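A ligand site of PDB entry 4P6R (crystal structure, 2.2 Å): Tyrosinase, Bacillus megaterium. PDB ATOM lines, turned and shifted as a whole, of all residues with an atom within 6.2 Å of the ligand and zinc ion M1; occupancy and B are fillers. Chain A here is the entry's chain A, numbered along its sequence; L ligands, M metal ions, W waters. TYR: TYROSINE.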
ATOM      1  N   HIS A  39     -23.628  -2.204   7.817  1.00  0.00           N
ATOM      2  CA  HIS A  39     -23.379  -3.420   8.585  1.00  0.00           C
ATOM      3  C   HIS A  39     -21.913  -3.584   8.932  1.00  0.00           C
ATOM      4  O   HIS A  39     -21.590  -3.928  10.065  1.00  0.00           O
ATOM      5  CB  HIS A  39     -23.869  -4.625   7.783  1.00  0.00           C
ATOM      6  CG  HIS A  39     -23.675  -5.942   8.453  1.00  0.00           C
ATOM      7  ND1 HIS A  39     -22.688  -6.825   8.079  1.00  0.00           N
ATOM      8  CD2 HIS A  39     -24.394  -6.574   9.426  1.00  0.00           C
ATOM      9  CE1 HIS A  39     -22.779  -7.929   8.810  1.00  0.00           C
ATOM     10  NE2 HIS A  39     -23.814  -7.807   9.623  1.00  0.00           N
ATOM     11  N   ALA A  56     -23.691  -4.272  16.292  1.00  0.00           N
ATOM     12  CA  ALA A  56     -24.608  -5.167  15.604  1.00  0.00           C
ATOM     13  C   ALA A  56     -24.470  -6.656  15.940  1.00  0.00           C
ATOM     14  O   ALA A  56     -25.293  -7.450  15.501  1.00  0.00           O
ATOM     15  CB  ALA A  56     -24.550  -4.961  14.099  1.00  0.00           C
ATOM     16  N   HIS A  57     -23.435  -7.046  16.675  1.00  0.00           N
ATOM     17  CA  HIS A  57     -23.142  -8.452  16.948  1.00  0.00           C
ATOM     18  C   HIS A  57     -22.565  -8.663  18.309  1.00  0.00           C
ATOM     19  O   HIS A  57     -22.039  -7.735  18.922  1.00  0.00           O
ATOM     20  CB  HIS A  57     -22.119  -9.052  15.974  1.00  0.00           C
ATOM     21  CG  HIS A  57     -22.362  -8.737  14.523  1.00  0.00           C
ATOM     22  ND1 HIS A  57     -21.983  -7.596  13.973  1.00  0.00           N
ATOM     23  CD2 HIS A  57     -22.934  -9.477  13.521  1.00  0.00           C
ATOM     24  CE1 HIS A  57     -22.312  -7.593  12.693  1.00  0.00           C
ATOM     25  NE2 HIS A  57     -22.894  -8.751  12.405  1.00  0.00           N
ATOM     26  N   MET A  58     -22.607  -9.903  18.778  1.00  0.00           N
ATOM     27  CA  MET A  58     -21.845 -10.322  19.965  1.00  0.00           C
ATOM     28  C   MET A  58     -22.259  -9.587  21.221  1.00  0.00           C
ATOM     29  O   MET A  58     -21.450  -9.324  22.091  1.00  0.00           O
ATOM     30  CB  MET A  58     -20.350 -10.176  19.724  1.00  0.00           C
ATOM     31  CG  MET A  58     -19.883 -10.911  18.496  1.00  0.00           C
ATOM     32  SD  MET A  58     -18.156 -10.773  18.083  1.00  0.00           S
ATOM     33  CE  MET A  58     -18.098 -11.852  16.678  1.00  0.00           C
ATOM     34  N   PHE A  62     -27.749  -7.269  19.063  1.00  0.00           N
ATOM     35  CA  PHE A  62     -27.668  -8.088  17.842  1.00  0.00           C
ATOM     36  C   PHE A  62     -29.033  -8.183  17.154  1.00  0.00           C
ATOM     37  O   PHE A  62     -29.137  -7.882  15.957  1.00  0.00           O
ATOM     38  CB  PHE A  62     -27.137  -9.471  18.170  1.00  0.00           C
ATOM     39  CG  PHE A  62     -27.356 -10.501  17.072  1.00  0.00           C
ATOM     40  CD1 PHE A  62     -26.681 -10.394  15.859  1.00  0.00           C
ATOM     41  CD2 PHE A  62     -28.204 -11.586  17.264  1.00  0.00           C
ATOM     42  CE1 PHE A  62     -26.879 -11.320  14.852  1.00  0.00           C
ATOM     43  CE2 PHE A  62     -28.409 -12.510  16.264  1.00  0.00           C
ATOM     44  CZ  PHE A  62     -27.747 -12.384  15.060  1.00  0.00           C
ATOM     45  N   HIS A  66     -30.544  -5.829  13.843  1.00  0.00           N
ATOM     46  CA  HIS A  66     -30.904  -6.458  12.582  1.00  0.00           C
ATOM     47  C   HIS A  66     -32.372  -6.300  12.188  1.00  0.00           C
ATOM     48  O   HIS A  66     -32.684  -6.281  10.997  1.00  0.00           O
ATOM     49  CB  HIS A  66     -30.454  -7.930  12.546  1.00  0.00           C
ATOM     50  CG  HIS A  66     -28.982  -8.102  12.347  1.00  0.00           C
ATOM     51  ND1 HIS A  66     -28.075  -7.993  13.372  1.00  0.00           N
ATOM     52  CD2 HIS A  66     -28.254  -8.352  11.227  1.00  0.00           C
ATOM     53  CE1 HIS A  66     -26.852  -8.178  12.901  1.00  0.00           C
ATOM     54  NE2 HIS A  66     -26.931  -8.408  11.605  1.00  0.00           N
ATOM     55  N   GLY A 193     -25.518 -17.513  18.136  1.00  0.00           N
ATOM     56  CA  GLY A 193     -24.834 -18.755  17.802  1.00  0.00           C
ATOM     57  C   GLY A 193     -23.559 -19.100  18.537  1.00  0.00           C
ATOM     58  O   GLY A 193     -22.815 -19.967  18.088  1.00  0.00           O
ATOM     59  N   PHE A 194     -23.314 -18.452  19.679  1.00  0.00           N
ATOM     60  CA  PHE A 194     -22.037 -18.634  20.366  1.00  0.00           C
ATOM     61  C   PHE A 194     -22.012 -19.743  21.430  1.00  0.00           C
ATOM     62  O   PHE A 194     -20.959 -20.087  21.963  1.00  0.00           O
ATOM     63  CB  PHE A 194     -21.532 -17.306  20.948  1.00  0.00           C
ATOM     64  CG  PHE A 194     -21.125 -16.317  19.902  1.00  0.00           C
ATOM     65  CD1 PHE A 194     -19.934 -16.487  19.203  1.00  0.00           C
ATOM     66  CD2 PHE A 194     -21.926 -15.228  19.594  1.00  0.00           C
ATOM     67  CE1 PHE A 194     -19.547 -15.580  18.230  1.00  0.00           C
ATOM     68  CE2 PHE A 194     -21.551 -14.312  18.620  1.00  0.00           C
ATOM     69  CZ  PHE A 194     -20.369 -14.493  17.931  1.00  0.00           C
ATOM     70  N   PRO A 198     -20.026 -22.734  16.126  1.00  0.00           N
ATOM     71  CA  PRO A 198     -21.133 -21.903  15.628  1.00  0.00           C
ATOM     72  C   PRO A 198     -22.457 -22.660  15.485  1.00  0.00           C
ATOM     73  O   PRO A 198     -22.508 -23.682  14.788  1.00  0.00           O
ATOM     74  CB  PRO A 198     -20.629 -21.456  14.259  1.00  0.00           C
ATOM     75  CG  PRO A 198     -19.821 -22.648  13.780  1.00  0.00           C
ATOM     76  CD  PRO A 198     -19.181 -23.237  15.022  1.00  0.00           C
ATOM     77  N   HIS A 201     -27.711 -18.818  13.888  1.00  0.00           N
ATOM     78  CA  HIS A 201     -27.395 -17.685  13.007  1.00  0.00           C
ATOM     79  C   HIS A 201     -25.978 -17.711  12.502  1.00  0.00           C
ATOM     80  O   HIS A 201     -25.765 -17.520  11.314  1.00  0.00           O
ATOM     81  CB  HIS A 201     -27.687 -16.322  13.665  1.00  0.00           C
ATOM     82  CG  HIS A 201     -26.873 -15.161  13.110  1.00  0.00           C
ATOM     83  ND1 HIS A 201     -25.694 -14.806  13.611  1.00  0.00           N
ATOM     84  CD2 HIS A 201     -27.139 -14.271  12.084  1.00  0.00           C
ATOM     85  CE1 HIS A 201     -25.223 -13.761  12.939  1.00  0.00           C
ATOM     86  NE2 HIS A 201     -26.105 -13.437  11.999  1.00  0.00           N
ATOM     87  N   ASN A 202     -25.019 -17.949  13.385  1.00  0.00           N
ATOM     88  CA  ASN A 202     -23.598 -17.975  13.023  1.00  0.00           C
ATOM     89  C   ASN A 202     -23.277 -19.140  12.100  1.00  0.00           C
ATOM     90  O   ASN A 202     -22.486 -19.006  11.145  1.00  0.00           O
ATOM     91  CB  ASN A 202     -22.717 -18.050  14.280  1.00  0.00           C
ATOM     92  CG  ASN A 202     -22.673 -16.730  15.066  1.00  0.00           C
ATOM     93  OD1 ASN A 202     -23.175 -15.699  14.619  1.00  0.00           O
ATOM     94  ND2 ASN A 202     -22.072 -16.767  16.260  1.00  0.00           N
ATOM     95  N   ARG A 203     -23.883 -20.288  12.385  1.00  0.00           N
ATOM     96  CA  ARG A 203     -23.648 -21.487  11.598  1.00  0.00           C
ATOM     97  C   ARG A 203     -24.149 -21.285  10.185  1.00  0.00           C
ATOM     98  O   ARG A 203     -23.485 -21.690   9.229  1.00  0.00           O
ATOM     99  CB  ARG A 203     -24.265 -22.724  12.233  1.00  0.00           C
ATOM    100  CG  ARG A 203     -24.118 -23.984  11.372  1.00  0.00           C
ATOM    101  CD  ARG A 203     -24.755 -25.175  12.058  1.00  0.00           C
ATOM    102  NE  ARG A 203     -23.941 -25.590  13.176  1.00  0.00           N
ATOM    103  CZ  ARG A 203     -23.238 -26.717  13.220  1.00  0.00           C
ATOM    104  NH1 ARG A 203     -23.297 -27.569  12.197  1.00  0.00           N
ATOM    105  NH2 ARG A 203     -22.513 -26.994  14.292  1.00  0.00           N
ATOM    106  N   HIS A 205     -24.263 -18.454   8.467  1.00  0.00           N
ATOM    107  CA  HIS A 205     -23.268 -17.633   7.801  1.00  0.00           C
ATOM    108  C   HIS A 205     -22.093 -18.466   7.260  1.00  0.00           C
ATOM    109  O   HIS A 205     -21.759 -18.382   6.080  1.00  0.00           O
ATOM    110  CB  HIS A 205     -22.743 -16.560   8.757  1.00  0.00           C
ATOM    111  CG  HIS A 205     -23.584 -15.318   8.807  1.00  0.00           C
ATOM    112  ND1 HIS A 205     -23.578 -14.374   7.798  1.00  0.00           N
ATOM    113  CD2 HIS A 205     -24.454 -14.857   9.745  1.00  0.00           C
ATOM    114  CE1 HIS A 205     -24.388 -13.378   8.123  1.00  0.00           C
ATOM    115  NE2 HIS A 205     -24.945 -13.660   9.290  1.00  0.00           N
ATOM    116  N   ARG A 206     -21.511 -19.289   8.130  1.00  0.00           N
ATOM    117  CA  ARG A 206     -20.336 -20.076   7.788  1.00  0.00           C
ATOM    118  C   ARG A 206     -20.639 -21.244   6.822  1.00  0.00           C
ATOM    119  O   ARG A 206     -19.769 -21.626   6.039  1.00  0.00           O
ATOM    120  CB  ARG A 206     -19.638 -20.599   9.053  1.00  0.00           C
ATOM    121  CG  ARG A 206     -19.747 -19.667  10.243  1.00  0.00           C
ATOM    122  CD  ARG A 206     -18.421 -19.275  10.893  1.00  0.00           C
ATOM    123  NE  ARG A 206     -17.648 -20.403  11.402  1.00  0.00           N
ATOM    124  CZ  ARG A 206     -17.002 -20.419  12.559  1.00  0.00           C
ATOM    125  NH1 ARG A 206     -17.064 -19.363  13.380  1.00  0.00           N
ATOM    126  NH2 ARG A 206     -16.306 -21.480  12.925  1.00  0.00           N
ATOM    127  N   GLN A 211     -18.652 -14.525   0.806  1.00  0.00           N
ATOM    128  CA  GLN A 211     -18.823 -13.300   1.577  1.00  0.00           C
ATOM    129  C   GLN A 211     -19.720 -13.487   2.809  1.00  0.00           C
ATOM    130  O   GLN A 211     -19.579 -12.740   3.779  1.00  0.00           O
ATOM    131  CB  GLN A 211     -19.370 -12.163   0.713  1.00  0.00           C
ATOM    132  CG  GLN A 211     -18.395 -11.573  -0.301  1.00  0.00           C
ATOM    133  CD  GLN A 211     -18.401 -12.359  -1.601  1.00  0.00           C
ATOM    134  OE1 GLN A 211     -19.075 -13.406  -1.710  1.00  0.00           O
ATOM    135  NE2 GLN A 211     -17.663 -11.867  -2.590  1.00  0.00           N
ATOM    136  N   MET A 212     -20.625 -14.471   2.804  1.00  0.00           N
ATOM    137  CA  MET A 212     -21.543 -14.690   3.932  1.00  0.00           C
ATOM    138  C   MET A 212     -20.821 -15.171   5.176  1.00  0.00           C
ATOM    139  O   MET A 212     -21.374 -15.137   6.282  1.00  0.00           O
ATOM    140  CB  MET A 212     -22.634 -15.702   3.577  1.00  0.00           C
ATOM    141  CG  MET A 212     -23.912 -15.073   3.018  1.00  0.00           C
ATOM    142  SD  MET A 212     -24.802 -14.032   4.210  1.00  0.00           S
ATOM    143  CE  MET A 212     -26.041 -15.196   4.836  1.00  0.00           C
ATOM    144  N   GLY A 213     -19.567 -15.602   5.009  1.00  0.00           N
ATOM    145  CA  GLY A 213     -18.827 -16.172   6.123  1.00  0.00           C
ATOM    146  C   GLY A 213     -18.068 -15.150   6.941  1.00  0.00           C
ATOM    147  O   GLY A 213     -17.468 -15.464   7.982  1.00  0.00           O
ATOM    148  N   VAL A 214     -18.067 -13.905   6.471  1.00  0.00           N
ATOM    149  CA  VAL A 214     -17.280 -12.867   7.143  1.00  0.00           C
ATOM    150  C   VAL A 214     -18.088 -11.594   7.373  1.00  0.00           C
ATOM    151  O   VAL A 214     -18.793 -11.108   6.486  1.00  0.00           O
ATOM    152  CB  VAL A 214     -15.892 -12.627   6.467  1.00  0.00           C
ATOM    153  CG1 VAL A 214     -15.564 -13.706   5.455  1.00  0.00           C
ATOM    154  CG2 VAL A 214     -15.799 -11.261   5.802  1.00  0.00           C
ATOM    155  N   VAL A 215     -17.991 -11.079   8.589  1.00  0.00           N
ATOM    156  CA  VAL A 215     -18.785  -9.907   8.999  1.00  0.00           C
ATOM    157  C   VAL A 215     -18.779  -8.731   8.004  1.00  0.00           C
ATOM    158  O   VAL A 215     -19.848  -8.347   7.529  1.00  0.00           O
ATOM    159  CB  VAL A 215     -18.444  -9.433  10.440  1.00  0.00           C
ATOM    160  CG1 VAL A 215     -19.385  -8.299  10.889  1.00  0.00           C
ATOM    161  CG2 VAL A 215     -18.516 -10.605  11.391  1.00  0.00           C
ATOM    162  N   PRO A 216     -17.587  -8.194   7.656  1.00  0.00           N
ATOM    163  CA  PRO A 216     -17.581  -6.987   6.804  1.00  0.00           C
ATOM    164  C   PRO A 216     -18.163  -7.121   5.392  1.00  0.00           C
ATOM    165  O   PRO A 216     -18.565  -6.119   4.803  1.00  0.00           O
ATOM    166  CB  PRO A 216     -16.102  -6.596   6.726  1.00  0.00           C
ATOM    167  CG  PRO A 216     -15.339  -7.748   7.249  1.00  0.00           C
ATOM    168  CD  PRO A 216     -16.245  -8.486   8.181  1.00  0.00           C
ATOM    169  N   ALA A 218     -20.490  -9.903   4.486  1.00  0.00           N
ATOM    170  CA  ALA A 218     -21.703 -10.744   4.437  1.00  0.00           C
ATOM    171  C   ALA A 218     -22.911 -10.210   3.639  1.00  0.00           C
ATOM    172  O   ALA A 218     -23.439 -10.920   2.797  1.00  0.00           O
ATOM    173  CB  ALA A 218     -22.110 -11.224   5.836  1.00  0.00           C
ATOM    174  N   PRO A 219     -23.291  -8.939   3.834  1.00  0.00           N
ATOM    175  CA  PRO A 219     -24.428  -8.405   3.067  1.00  0.00           C
ATOM    176  C   PRO A 219     -24.228  -8.259   1.543  1.00  0.00           C
ATOM    177  O   PRO A 219     -25.219  -7.948   0.858  1.00  0.00           O
ATOM    178  CB  PRO A 219     -24.656  -7.017   3.709  1.00  0.00           C
ATOM    179  CG  PRO A 219     -24.154  -7.196   5.098  1.00  0.00           C
ATOM    180  CD  PRO A 219     -22.936  -8.046   4.951  1.00  0.00           C
ATOM    181  N   PHE A 224     -28.350 -12.846   2.653  1.00  0.00           N
ATOM    182  CA  PHE A 224     -28.124 -12.306   3.988  1.00  0.00           C
ATOM    183  C   PHE A 224     -29.451 -11.855   4.576  1.00  0.00           C
ATOM    184  O   PHE A 224     -29.722 -12.089   5.748  1.00  0.00           O
ATOM    185  CB  PHE A 224     -27.158 -11.108   3.912  1.00  0.00           C
ATOM    186  CG  PHE A 224     -26.894 -10.449   5.240  1.00  0.00           C
ATOM    187  CD1 PHE A 224     -27.737  -9.476   5.738  1.00  0.00           C
ATOM    188  CD2 PHE A 224     -25.756 -10.776   5.985  1.00  0.00           C
ATOM    189  CE1 PHE A 224     -27.491  -8.846   6.980  1.00  0.00           C
ATOM    190  CE2 PHE A 224     -25.478 -10.138   7.214  1.00  0.00           C
ATOM    191  CZ  PHE A 224     -26.362  -9.184   7.705  1.00  0.00           C
ATOM    192  N   HIS A 228     -31.604 -13.278   7.713  1.00  0.00           N
ATOM    193  CA  HIS A 228     -31.970 -12.485   8.875  1.00  0.00           C
ATOM    194  C   HIS A 228     -33.473 -12.341   9.099  1.00  0.00           C
ATOM    195  O   HIS A 228     -33.932 -12.263  10.245  1.00  0.00           O
ATOM    196  CB  HIS A 228     -31.202 -11.155   8.929  1.00  0.00           C
ATOM    197  CG  HIS A 228     -29.833 -11.328   9.497  1.00  0.00           C
ATOM    198  ND1 HIS A 228     -29.598 -11.321  10.856  1.00  0.00           N
ATOM    199  CD2 HIS A 228     -28.658 -11.651   8.906  1.00  0.00           C
ATOM    200  CE1 HIS A 228     -28.310 -11.572  11.072  1.00  0.00           C
ATOM    201  NE2 HIS A 228     -27.724 -11.788   9.905  1.00  0.00           N
HETATM  202  N   TYR L   1     -18.900 -14.345  13.480  1.00  0.00           N
HETATM  203  CA  TYR L   1     -19.737 -15.500  13.171  1.00  0.00           C
HETATM  204  C   TYR L   1     -19.075 -16.760  13.718  1.00  0.00           C
HETATM  205  O   TYR L   1     -19.602 -17.880  13.677  1.00  0.00           O
HETATM  206  CB  TYR L   1     -19.992 -15.598  11.658  1.00  0.00           C
HETATM  207  CG  TYR L   1     -20.690 -14.375  11.101  1.00  0.00           C
HETATM  208  CD1 TYR L   1     -21.585 -13.653  11.874  1.00  0.00           C
HETATM  209  CD2 TYR L   1     -20.448 -13.930   9.797  1.00  0.00           C
HETATM  210  CE1 TYR L   1     -22.232 -12.535  11.385  1.00  0.00           C
HETATM  211  CE2 TYR L   1     -21.100 -12.783   9.306  1.00  0.00           C
HETATM  212  CZ  TYR L   1     -21.993 -12.103  10.114  1.00  0.00           C
HETATM  213  OH  TYR L   1     -22.668 -10.993   9.691  1.00  0.00           O
HETATM  214  OXT TYR L   1     -17.973 -16.642  14.260  1.00  0.00           O
HETATM  215 ZN    ZN M   1     -23.534  -9.596  10.657  1.00  0.00          ZN
HETATM  216 ZN    ZN M   2     -25.860 -12.199  10.470  1.00  0.00          ZN
HETATM  217  O   HOH W   1     -19.900 -12.128  14.555  1.00  0.00           O
HETATM  218  O   HOH W   2     -19.895 -19.003  16.593  1.00  0.00           O
HETATM  219  O   HOH W   3     -25.429 -10.156  10.744  1.00  0.00           O
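An oxygen (O) of the ligand lies within salt-bridge range of the guanidinium group (NH1) of Arg 206 (3.0 Å).
A ring nitrogen (ND1) of His 39 lies close to the backbone carbonyl oxygen of Val 215, 3.3 Å away.
The side-chain amide oxygen (OD1) of Asn 202 is in hydrogen-bond range of a ring nitrogen (ND1) of His 201 (2.9 Å).
The backbone carbonyl oxygen (O) of Met 212 lies within hydrogen-bond range of a ring nitrogen (ND1) of His 205, at 2.8 Å.
A ring nitrogen (ND1) of His 66 is in hydrogen-bond range of the backbone carbonyl oxygen (O) of Phe 62 (2.8 Å).
The backbone carbonyl oxygen of Pro 198 sits at hydrogen-bond distance from the guanidinium group of Arg 203 (2.9 Å).
The backbone carbonyl oxygen (O) of Gln 211 lies close to the backbone NH (N) of Ala 218, at 3.1 Å.
Residues that only touch the ligand: Pro 198, His 201, Asn 202, His 205, Met 212, Gly 213, Val 214, Val 215, Ala 218 and Phe 224.
Hydrophobic or aromatic side chains that line the ligand: His 39, His 57, Pro 198, His 201, His 205, Val 215, Ala 218 and Phe 224.
13 residues have an atom within 4 Å of the ligand: His 39, His 57, Pro 198, His 201, Asn 202, His 205, Arg 206, Met 212, Gly 213, Val 214, Val 215, Ala 218 and Phe 224.
Along chain A the residues within 4 Å of the ligand span positions 39 to 224.
The nearest printed residue that does not touch the ligand is Met 58 (4.1 Å).
Merely in contact with zinc ion M1: His 66 and Phe 224.
Of the 24 residues printed, 4 come within 4 Å of zinc ion M1.
The nearest printed residue that does not touch zinc ion M1 is Val 215 (4.4 Å).
Zinc ion M1 is bound by an oxygen (OH) of the ligand, water W3, a ring nitrogen (NE2) of His 57 and a ring nitrogen (NE2) of His 39.
Zinc ion M1 has four donor atoms within binding distance.
Water W2 lies within hydrogen-bond range of O of the ligand (3.1 Å), ND2 of Asn 202 (3.1 Å) and O of Gly 193 (3.4 Å).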
